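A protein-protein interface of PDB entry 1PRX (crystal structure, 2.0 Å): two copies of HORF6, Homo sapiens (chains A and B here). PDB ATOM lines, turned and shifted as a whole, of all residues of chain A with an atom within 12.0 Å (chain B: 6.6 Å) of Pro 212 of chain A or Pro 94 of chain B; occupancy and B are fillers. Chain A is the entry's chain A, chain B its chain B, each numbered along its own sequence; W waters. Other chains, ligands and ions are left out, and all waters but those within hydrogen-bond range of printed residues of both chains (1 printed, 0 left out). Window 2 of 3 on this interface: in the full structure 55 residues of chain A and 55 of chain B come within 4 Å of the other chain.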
ATOM      1  N   THR A 208      28.182   7.001  34.270  1.00  0.00           N
ATOM      2  CA  THR A 208      28.410   8.126  33.373  1.00  0.00           C
ATOM      3  C   THR A 208      28.788   7.594  31.995  1.00  0.00           C
ATOM      4  O   THR A 208      29.833   6.962  31.838  1.00  0.00           O
ATOM      5  CB  THR A 208      29.545   9.032  33.882  1.00  0.00           C
ATOM      6  OG1 THR A 208      29.279   9.418  35.237  1.00  0.00           O
ATOM      7  CG2 THR A 208      29.674  10.281  33.012  1.00  0.00           C
ATOM      8  N   LYS A 209      27.926   7.803  31.007  1.00  0.00           N
ATOM      9  CA  LYS A 209      28.229   7.335  29.670  1.00  0.00           C
ATOM     10  C   LYS A 209      29.249   8.305  29.074  1.00  0.00           C
ATOM     11  O   LYS A 209      29.013   9.507  29.028  1.00  0.00           O
ATOM     12  CB  LYS A 209      26.958   7.278  28.822  1.00  0.00           C
ATOM     13  CG  LYS A 209      27.169   6.707  27.425  1.00  0.00           C
ATOM     14  CD  LYS A 209      25.866   6.172  26.838  1.00  0.00           C
ATOM     15  CE  LYS A 209      26.026   5.679  25.396  1.00  0.00           C
ATOM     16  NZ  LYS A 209      27.053   4.618  25.231  1.00  0.00           N
ATOM     17  N   GLU A 210      30.399   7.792  28.658  1.00  0.00           N
ATOM     18  CA  GLU A 210      31.418   8.659  28.084  1.00  0.00           C
ATOM     19  C   GLU A 210      31.056   9.143  26.683  1.00  0.00           C
ATOM     20  O   GLU A 210      30.696   8.345  25.817  1.00  0.00           O
ATOM     21  CB  GLU A 210      32.782   7.968  28.092  1.00  0.00           C
ATOM     22  CG  GLU A 210      33.433   7.946  29.462  1.00  0.00           C
ATOM     23  CD  GLU A 210      33.440   9.320  30.131  1.00  0.00           C
ATOM     24  OE1 GLU A 210      33.846  10.314  29.477  1.00  0.00           O
ATOM     25  OE2 GLU A 210      33.025   9.401  31.313  1.00  0.00           O
ATOM     26  N   LEU A 211      31.115  10.456  26.477  1.00  0.00           N
ATOM     27  CA  LEU A 211      30.787  11.048  25.186  1.00  0.00           C
ATOM     28  C   LEU A 211      31.989  11.718  24.536  1.00  0.00           C
ATOM     29  O   LEU A 211      32.946  12.080  25.218  1.00  0.00           O
ATOM     30  CB  LEU A 211      29.666  12.080  25.330  1.00  0.00           C
ATOM     31  CG  LEU A 211      28.214  11.638  25.530  1.00  0.00           C
ATOM     32  CD1 LEU A 211      27.985  10.231  24.986  1.00  0.00           C
ATOM     33  CD2 LEU A 211      27.890  11.690  26.986  1.00  0.00           C
ATOM     34  N   PRO A 212      31.938  11.921  23.206  1.00  0.00           N
ATOM     35  CA  PRO A 212      33.009  12.558  22.435  1.00  0.00           C
ATOM     36  C   PRO A 212      33.470  13.887  23.020  1.00  0.00           C
ATOM     37  O   PRO A 212      34.633  14.258  22.870  1.00  0.00           O
ATOM     38  CB  PRO A 212      32.355  12.773  21.071  1.00  0.00           C
ATOM     39  CG  PRO A 212      31.523  11.569  20.942  1.00  0.00           C
ATOM     40  CD  PRO A 212      30.870  11.460  22.301  1.00  0.00           C
ATOM     41  N   SER A 213      32.569  14.586  23.704  1.00  0.00           N
ATOM     42  CA  SER A 213      32.889  15.888  24.277  1.00  0.00           C
ATOM     43  C   SER A 213      33.641  15.882  25.619  1.00  0.00           C
ATOM     44  O   SER A 213      34.117  16.927  26.083  1.00  0.00           O
ATOM     45  CB  SER A 213      31.606  16.720  24.403  1.00  0.00           C
ATOM     46  OG  SER A 213      30.787  16.244  25.457  1.00  0.00           O
ATOM     47  N   GLY A 214      33.733  14.726  26.261  1.00  0.00           N
ATOM     48  CA  GLY A 214      34.410  14.674  27.547  1.00  0.00           C
ATOM     49  C   GLY A 214      33.538  15.170  28.696  1.00  0.00           C
ATOM     50  O   GLY A 214      33.907  15.028  29.864  1.00  0.00           O
ATOM     51  N   LYS A 215      32.371  15.724  28.369  1.00  0.00           N
ATOM     52  CA  LYS A 215      31.452  16.212  29.387  1.00  0.00           C
ATOM     53  C   LYS A 215      30.751  15.033  30.032  1.00  0.00           C
ATOM     54  O   LYS A 215      30.477  14.021  29.382  1.00  0.00           O
ATOM     55  CB  LYS A 215      30.448  17.193  28.799  1.00  0.00           C
ATOM     56  CG  LYS A 215      31.118  18.435  28.259  1.00  0.00           C
ATOM     57  CD  LYS A 215      30.125  19.488  27.849  1.00  0.00           C
ATOM     58  CE  LYS A 215      30.839  20.680  27.254  1.00  0.00           C
ATOM     59  NZ  LYS A 215      29.869  21.713  26.811  1.00  0.00           N
ATOM     60  N   LYS A 216      30.480  15.174  31.324  1.00  0.00           N
ATOM     61  CA  LYS A 216      29.853  14.122  32.098  1.00  0.00           C
ATOM     62  C   LYS A 216      28.424  14.441  32.532  1.00  0.00           C
ATOM     63  O   LYS A 216      28.116  14.410  33.718  1.00  0.00           O
ATOM     64  CB  LYS A 216      30.736  13.818  33.313  1.00  0.00           C
ATOM     65  CG  LYS A 216      32.114  13.253  32.946  1.00  0.00           C
ATOM     66  CD  LYS A 216      33.047  13.211  34.133  1.00  0.00           C
ATOM     67  CE  LYS A 216      33.442  14.618  34.564  1.00  0.00           C
ATOM     68  NZ  LYS A 216      34.256  14.603  35.821  1.00  0.00           N
ATOM     69  N   TYR A 217      27.547  14.692  31.562  1.00  0.00           N
ATOM     70  CA  TYR A 217      26.146  15.013  31.830  1.00  0.00           C
ATOM     71  C   TYR A 217      25.179  13.839  31.620  1.00  0.00           C
ATOM     72  O   TYR A 217      24.026  13.903  32.043  1.00  0.00           O
ATOM     73  CB  TYR A 217      25.712  16.207  30.986  1.00  0.00           C
ATOM     74  CG  TYR A 217      25.843  15.968  29.503  1.00  0.00           C
ATOM     75  CD1 TYR A 217      24.788  15.422  28.769  1.00  0.00           C
ATOM     76  CD2 TYR A 217      27.018  16.281  28.832  1.00  0.00           C
ATOM     77  CE1 TYR A 217      24.896  15.194  27.401  1.00  0.00           C
ATOM     78  CE2 TYR A 217      27.142  16.054  27.456  1.00  0.00           C
ATOM     79  CZ  TYR A 217      26.074  15.512  26.752  1.00  0.00           C
ATOM     80  OH  TYR A 217      26.165  15.297  25.407  1.00  0.00           O
ATOM     81  N   LEU A 218      25.611  12.790  30.920  1.00  0.00           N
ATOM     82  CA  LEU A 218      24.743  11.629  30.708  1.00  0.00           C
ATOM     83  C   LEU A 218      24.953  10.627  31.811  1.00  0.00           C
ATOM     84  O   LEU A 218      25.606   9.594  31.617  1.00  0.00           O
ATOM     85  CB  LEU A 218      24.997  10.919  29.379  1.00  0.00           C
ATOM     86  CG  LEU A 218      24.214  11.317  28.132  1.00  0.00           C
ATOM     87  CD1 LEU A 218      24.079  10.069  27.277  1.00  0.00           C
ATOM     88  CD2 LEU A 218      22.840  11.888  28.455  1.00  0.00           C
ATOM     89  N   ALA B  81      29.103  20.499  17.885  1.00  0.00           N
ATOM     90  CA  ALA B  81      29.823  19.642  18.823  1.00  0.00           C
ATOM     91  C   ALA B  81      28.840  18.705  19.530  1.00  0.00           C
ATOM     92  O   ALA B  81      29.085  17.505  19.658  1.00  0.00           O
ATOM     93  CB  ALA B  81      30.567  20.489  19.837  1.00  0.00           C
ATOM     94  N   SER B  83      26.204  17.497  18.387  1.00  0.00           N
ATOM     95  CA  SER B  83      25.787  16.466  17.430  1.00  0.00           C
ATOM     96  C   SER B  83      26.673  15.230  17.456  1.00  0.00           C
ATOM     97  O   SER B  83      26.197  14.123  17.212  1.00  0.00           O
ATOM     98  CB  SER B  83      25.712  17.035  16.015  1.00  0.00           C
ATOM     99  OG  SER B  83      24.690  18.008  15.958  1.00  0.00           O
ATOM    100  N   LYS B  84      27.951  15.392  17.785  1.00  0.00           N
ATOM    101  CA  LYS B  84      28.842  14.234  17.854  1.00  0.00           C
ATOM    102  C   LYS B  84      28.435  13.385  19.053  1.00  0.00           C
ATOM    103  O   LYS B  84      28.506  12.157  19.007  1.00  0.00           O
ATOM    104  CB  LYS B  84      30.295  14.674  18.002  1.00  0.00           C
ATOM    105  CG  LYS B  84      30.723  15.745  17.023  1.00  0.00           C
ATOM    106  CD  LYS B  84      32.214  15.670  16.775  1.00  0.00           C
ATOM    107  CE  LYS B  84      32.996  15.605  18.078  1.00  0.00           C
ATOM    108  NZ  LYS B  84      34.458  15.345  17.842  1.00  0.00           N
ATOM    109  N   ASP B  85      28.033  14.052  20.133  1.00  0.00           N
ATOM    110  CA  ASP B  85      27.570  13.388  21.355  1.00  0.00           C
ATOM    111  C   ASP B  85      26.277  12.636  21.058  1.00  0.00           C
ATOM    112  O   ASP B  85      26.154  11.456  21.394  1.00  0.00           O
ATOM    113  CB  ASP B  85      27.352  14.413  22.486  1.00  0.00           C
ATOM    114  CG  ASP B  85      28.648  14.785  23.206  1.00  0.00           C
ATOM    115  OD1 ASP B  85      29.739  14.346  22.773  1.00  0.00           O
ATOM    116  OD2 ASP B  85      28.573  15.500  24.228  1.00  0.00           O
ATOM    117  N   ILE B  86      25.330  13.314  20.406  1.00  0.00           N
ATOM    118  CA  ILE B  86      24.049  12.717  20.007  1.00  0.00           C
ATOM    119  C   ILE B  86      24.298  11.473  19.129  1.00  0.00           C
ATOM    120  O   ILE B  86      23.697  10.412  19.334  1.00  0.00           O
ATOM    121  CB  ILE B  86      23.185  13.731  19.218  1.00  0.00           C
ATOM    122  CG1 ILE B  86      22.905  14.977  20.076  1.00  0.00           C
ATOM    123  CG2 ILE B  86      21.892  13.065  18.762  1.00  0.00           C
ATOM    124  CD1 ILE B  86      22.227  16.135  19.326  1.00  0.00           C
ATOM    125  N   ASN B  87      25.194  11.612  18.155  1.00  0.00           N
ATOM    126  CA  ASN B  87      25.560  10.507  17.273  1.00  0.00           C
ATOM    127  C   ASN B  87      26.145   9.364  18.080  1.00  0.00           C
ATOM    128  O   ASN B  87      25.758   8.215  17.882  1.00  0.00           O
ATOM    129  CB  ASN B  87      26.578  10.950  16.208  1.00  0.00           C
ATOM    130  CG  ASN B  87      25.916  11.610  15.003  1.00  0.00           C
ATOM    131  OD1 ASN B  87      26.414  12.598  14.460  1.00  0.00           O
ATOM    132  ND2 ASN B  87      24.787  11.065  14.582  1.00  0.00           N
ATOM    133  N   ALA B  88      27.051   9.690  19.006  1.00  0.00           N
ATOM    134  CA  ALA B  88      27.709   8.705  19.869  1.00  0.00           C
ATOM    135  C   ALA B  88      26.726   8.010  20.810  1.00  0.00           C
ATOM    136  O   ALA B  88      26.862   6.820  21.100  1.00  0.00           O
ATOM    137  CB  ALA B  88      28.818   9.353  20.656  1.00  0.00           C
ATOM    138  N   TYR B  89      25.740   8.754  21.289  1.00  0.00           N
ATOM    139  CA  TYR B  89      24.722   8.186  22.155  1.00  0.00           C
ATOM    140  C   TYR B  89      23.939   7.124  21.349  1.00  0.00           C
ATOM    141  O   TYR B  89      23.571   6.076  21.874  1.00  0.00           O
ATOM    142  CB  TYR B  89      23.799   9.302  22.668  1.00  0.00           C
ATOM    143  CG  TYR B  89      22.473   8.815  23.212  1.00  0.00           C
ATOM    144  CD1 TYR B  89      22.349   8.387  24.535  1.00  0.00           C
ATOM    145  CD2 TYR B  89      21.338   8.786  22.396  1.00  0.00           C
ATOM    146  CE1 TYR B  89      21.122   7.941  25.035  1.00  0.00           C
ATOM    147  CE2 TYR B  89      20.116   8.348  22.882  1.00  0.00           C
ATOM    148  CZ  TYR B  89      20.008   7.926  24.198  1.00  0.00           C
ATOM    149  OH  TYR B  89      18.781   7.504  24.666  1.00  0.00           O
ATOM    150  N   GLU B  92      26.535   5.619  16.914  1.00  0.00           N
ATOM    151  CA  GLU B  92      26.845   5.906  15.524  1.00  0.00           C
ATOM    152  C   GLU B  92      28.178   6.628  15.434  1.00  0.00           C
ATOM    153  O   GLU B  92      28.737   7.055  16.447  1.00  0.00           O
ATOM    154  CB  GLU B  92      25.754   6.792  14.911  1.00  0.00           C
ATOM    155  CG  GLU B  92      24.952   6.145  13.801  1.00  0.00           C
ATOM    156  CD  GLU B  92      23.764   5.365  14.313  1.00  0.00           C
ATOM    157  OE1 GLU B  92      23.025   5.912  15.155  1.00  0.00           O
ATOM    158  OE2 GLU B  92      23.540   4.227  13.845  1.00  0.00           O
ATOM    159  N   GLU B  93      28.671   6.788  14.212  1.00  0.00           N
ATOM    160  CA  GLU B  93      29.917   7.490  13.981  1.00  0.00           C
ATOM    161  C   GLU B  93      29.692   8.898  14.536  1.00  0.00           C
ATOM    162  O   GLU B  93      28.739   9.578  14.153  1.00  0.00           O
ATOM    163  CB  GLU B  93      30.184   7.555  12.477  1.00  0.00           C
ATOM    164  CG  GLU B  93      31.616   7.309  12.068  1.00  0.00           C
ATOM    165  CD  GLU B  93      31.881   7.756  10.635  1.00  0.00           C
ATOM    166  OE1 GLU B  93      31.194   7.261   9.710  1.00  0.00           O
ATOM    167  OE2 GLU B  93      32.773   8.613  10.446  1.00  0.00           O
ATOM    168  N   PRO B  94      30.524   9.325  15.495  1.00  0.00           N
ATOM    169  CA  PRO B  94      30.408  10.649  16.108  1.00  0.00           C
ATOM    170  C   PRO B  94      30.754  11.775  15.155  1.00  0.00           C
ATOM    171  O   PRO B  94      31.804  12.406  15.270  1.00  0.00           O
ATOM    172  CB  PRO B  94      31.388  10.567  17.276  1.00  0.00           C
ATOM    173  CG  PRO B  94      32.445   9.674  16.742  1.00  0.00           C
ATOM    174  CD  PRO B  94      31.644   8.575  16.082  1.00  0.00           C
ATOM    175  N   THR B  95      29.843  12.027  14.226  1.00  0.00           N
ATOM    176  CA  THR B  95      29.986  13.070  13.223  1.00  0.00           C
ATOM    177  C   THR B  95      29.191  14.313  13.656  1.00  0.00           C
ATOM    178  O   THR B  95      28.426  14.268  14.618  1.00  0.00           O
ATOM    179  CB  THR B  95      29.417  12.571  11.882  1.00  0.00           C
ATOM    180  OG1 THR B  95      30.004  11.308  11.560  1.00  0.00           O
ATOM    181  CG2 THR B  95      29.707  13.556  10.759  1.00  0.00           C
ATOM    182  N   GLU B  96      29.396  15.430  12.964  1.00  0.00           N
ATOM    183  CA  GLU B  96      28.661  16.645  13.268  1.00  0.00           C
ATOM    184  C   GLU B  96      27.407  16.713  12.388  1.00  0.00           C
ATOM    185  O   GLU B  96      26.707  17.719  12.382  1.00  0.00           O
ATOM    186  CB  GLU B  96      29.512  17.885  13.006  1.00  0.00           C
ATOM    187  CG  GLU B  96      30.798  17.991  13.806  1.00  0.00           C
ATOM    188  CD  GLU B  96      31.554  19.284  13.520  1.00  0.00           C
ATOM    189  OE1 GLU B  96      31.411  19.833  12.405  1.00  0.00           O
ATOM    190  OE2 GLU B  96      32.289  19.770  14.407  1.00  0.00           O
ATOM    191  N   LYS B  97      27.131  15.659  11.627  1.00  0.00           N
ATOM    192  CA  LYS B  97      25.961  15.674  10.765  1.00  0.00           C
ATOM    193  C   LYS B  97      24.753  14.968  11.398  1.00  0.00           C
ATOM    194  O   LYS B  97      24.874  13.862  11.924  1.00  0.00           O
ATOM    195  CB  LYS B  97      26.315  15.072   9.400  1.00  0.00           C
ATOM    196  CG  LYS B  97      25.322  15.438   8.311  1.00  0.00           C
ATOM    197  CD  LYS B  97      25.910  15.313   6.906  1.00  0.00           C
ATOM    198  CE  LYS B  97      25.066  16.074   5.868  1.00  0.00           C
ATOM    199  NZ  LYS B  97      23.595  15.798   5.962  1.00  0.00           N
HETATM  200  O   HOH W   1      31.816  16.404  21.047  1.00  0.00           O
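Water W1 lies within hydrogen-bond range of O of Ala 81 of chain B (3.3 Å), N of Ser 213 of chain A (3.3 Å) and OD1 of Asp 85 of chain B (3.4 Å).
The backbone NH (N) of Lys 209 of chain A lies within hydrogen-bond range of the backbone carbonyl oxygen (O) of Leu 218 of chain A (3.0 Å).
O of Thr 95 of chain B lies close to N of Lys 84 of chain B.
OG of Ser 213 of chain A sits close to N of Lys 215 of chain A (3.4 Å).
No position is printed for both chains.
Printed residues of chain B that touch a printed residue of chain A: Lys 84, Asp 85, Ala 88, Tyr 89 and Pro 94.
Hydrophobic or aromatic side chains of chain B that line the printed part of chain A: Ala 88, Tyr 89 and Pro 94.
Of the 11 printed residues of chain A, 5 touch a printed residue of chain B.
Hydrophobic or aromatic side chains of chain A within 4 Å of the printed part of chain B: Leu 211, Pro 212, Tyr 217 and Leu 218.
Along chain A the printed residues that touch a printed residue of chain B span positions 211 to 218.
Among the printed residues, no Asp or Glu carboxylate lies within 4 Å of a Lys or Arg side-chain nitrogen of the other chain.
Among the printed residues, merely in contact across the chains: Pro 212 of chain A with Ala 88 of chain B (3.4 Å), Leu 211 of chain A with Asp 85 of chain B (3.4 Å), Pro 212 of chain A with Lys 84 of chain B (3.6 Å), Leu 218 of chain A with Tyr 89 of chain B (3.7 Å) and Pro 212 of chain A with Pro 94 of chain B (3.8 Å).
Of chain B, only Lys 84, Asp 85, Ala 88 and Pro 94 come within 4 Å of Pro 212 of chain A.
Of chain A, only Pro 212 comes within 4 Å of Lys 84 of chain B.
Of chain A, only Leu 211 (3.4 Å), Pro 212 (3.1 Å), Ser 213 (2.6 Å) and Tyr 217 (2.7 Å) come within 4 Å of Asp 85 of chain B.
No residue of chain A comes within 4 Å of Asn 87 of chain B.
Of chain A, only Pro 212 (3.4 Å) comes within 4 Å of Ala 88 of chain B.
No residue of chain A comes within 4 Å of Glu 93 of chain B.
Thr 95 of chain B touches none of the printed residues of chain A.
Of the printed residues of chain B, Leu 218 of chain A touches Tyr 89.
Printed residues of chain B within 4 Å of Leu 211 of chain A: Asp 85 (3.4 Å).
Of the printed residues of chain A, Tyr 89 of chain B touches Leu 218 (3.7 Å).
Printed residues of chain B within 4 Å of Ser 213 of chain A: Asp 85.
Of the printed residues of chain B, Tyr 217 of chain A touches Asp 85.
The nearest residue of chain A that does not touch Pro 94 of chain B is Leu 211 of chain A (7.4 Å).
The backbone nitrogen of Pro 212 of chain A lies close to the side-chain carboxylate of Asp 85 of chain B (3.3 Å).
The side-chain hydroxyl (OG) of Ser 213 of chain A sits at hydrogen-bond distance from the side-chain carboxylate (OD2) of Asp 85 of chain B, 2.6 Å away.
The side-chain hydroxyl (OH) of Tyr 217 of chain A sits at hydrogen-bond distance from the side-chain carboxylate (OD2) of Asp 85 of chain B (2.7 Å).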
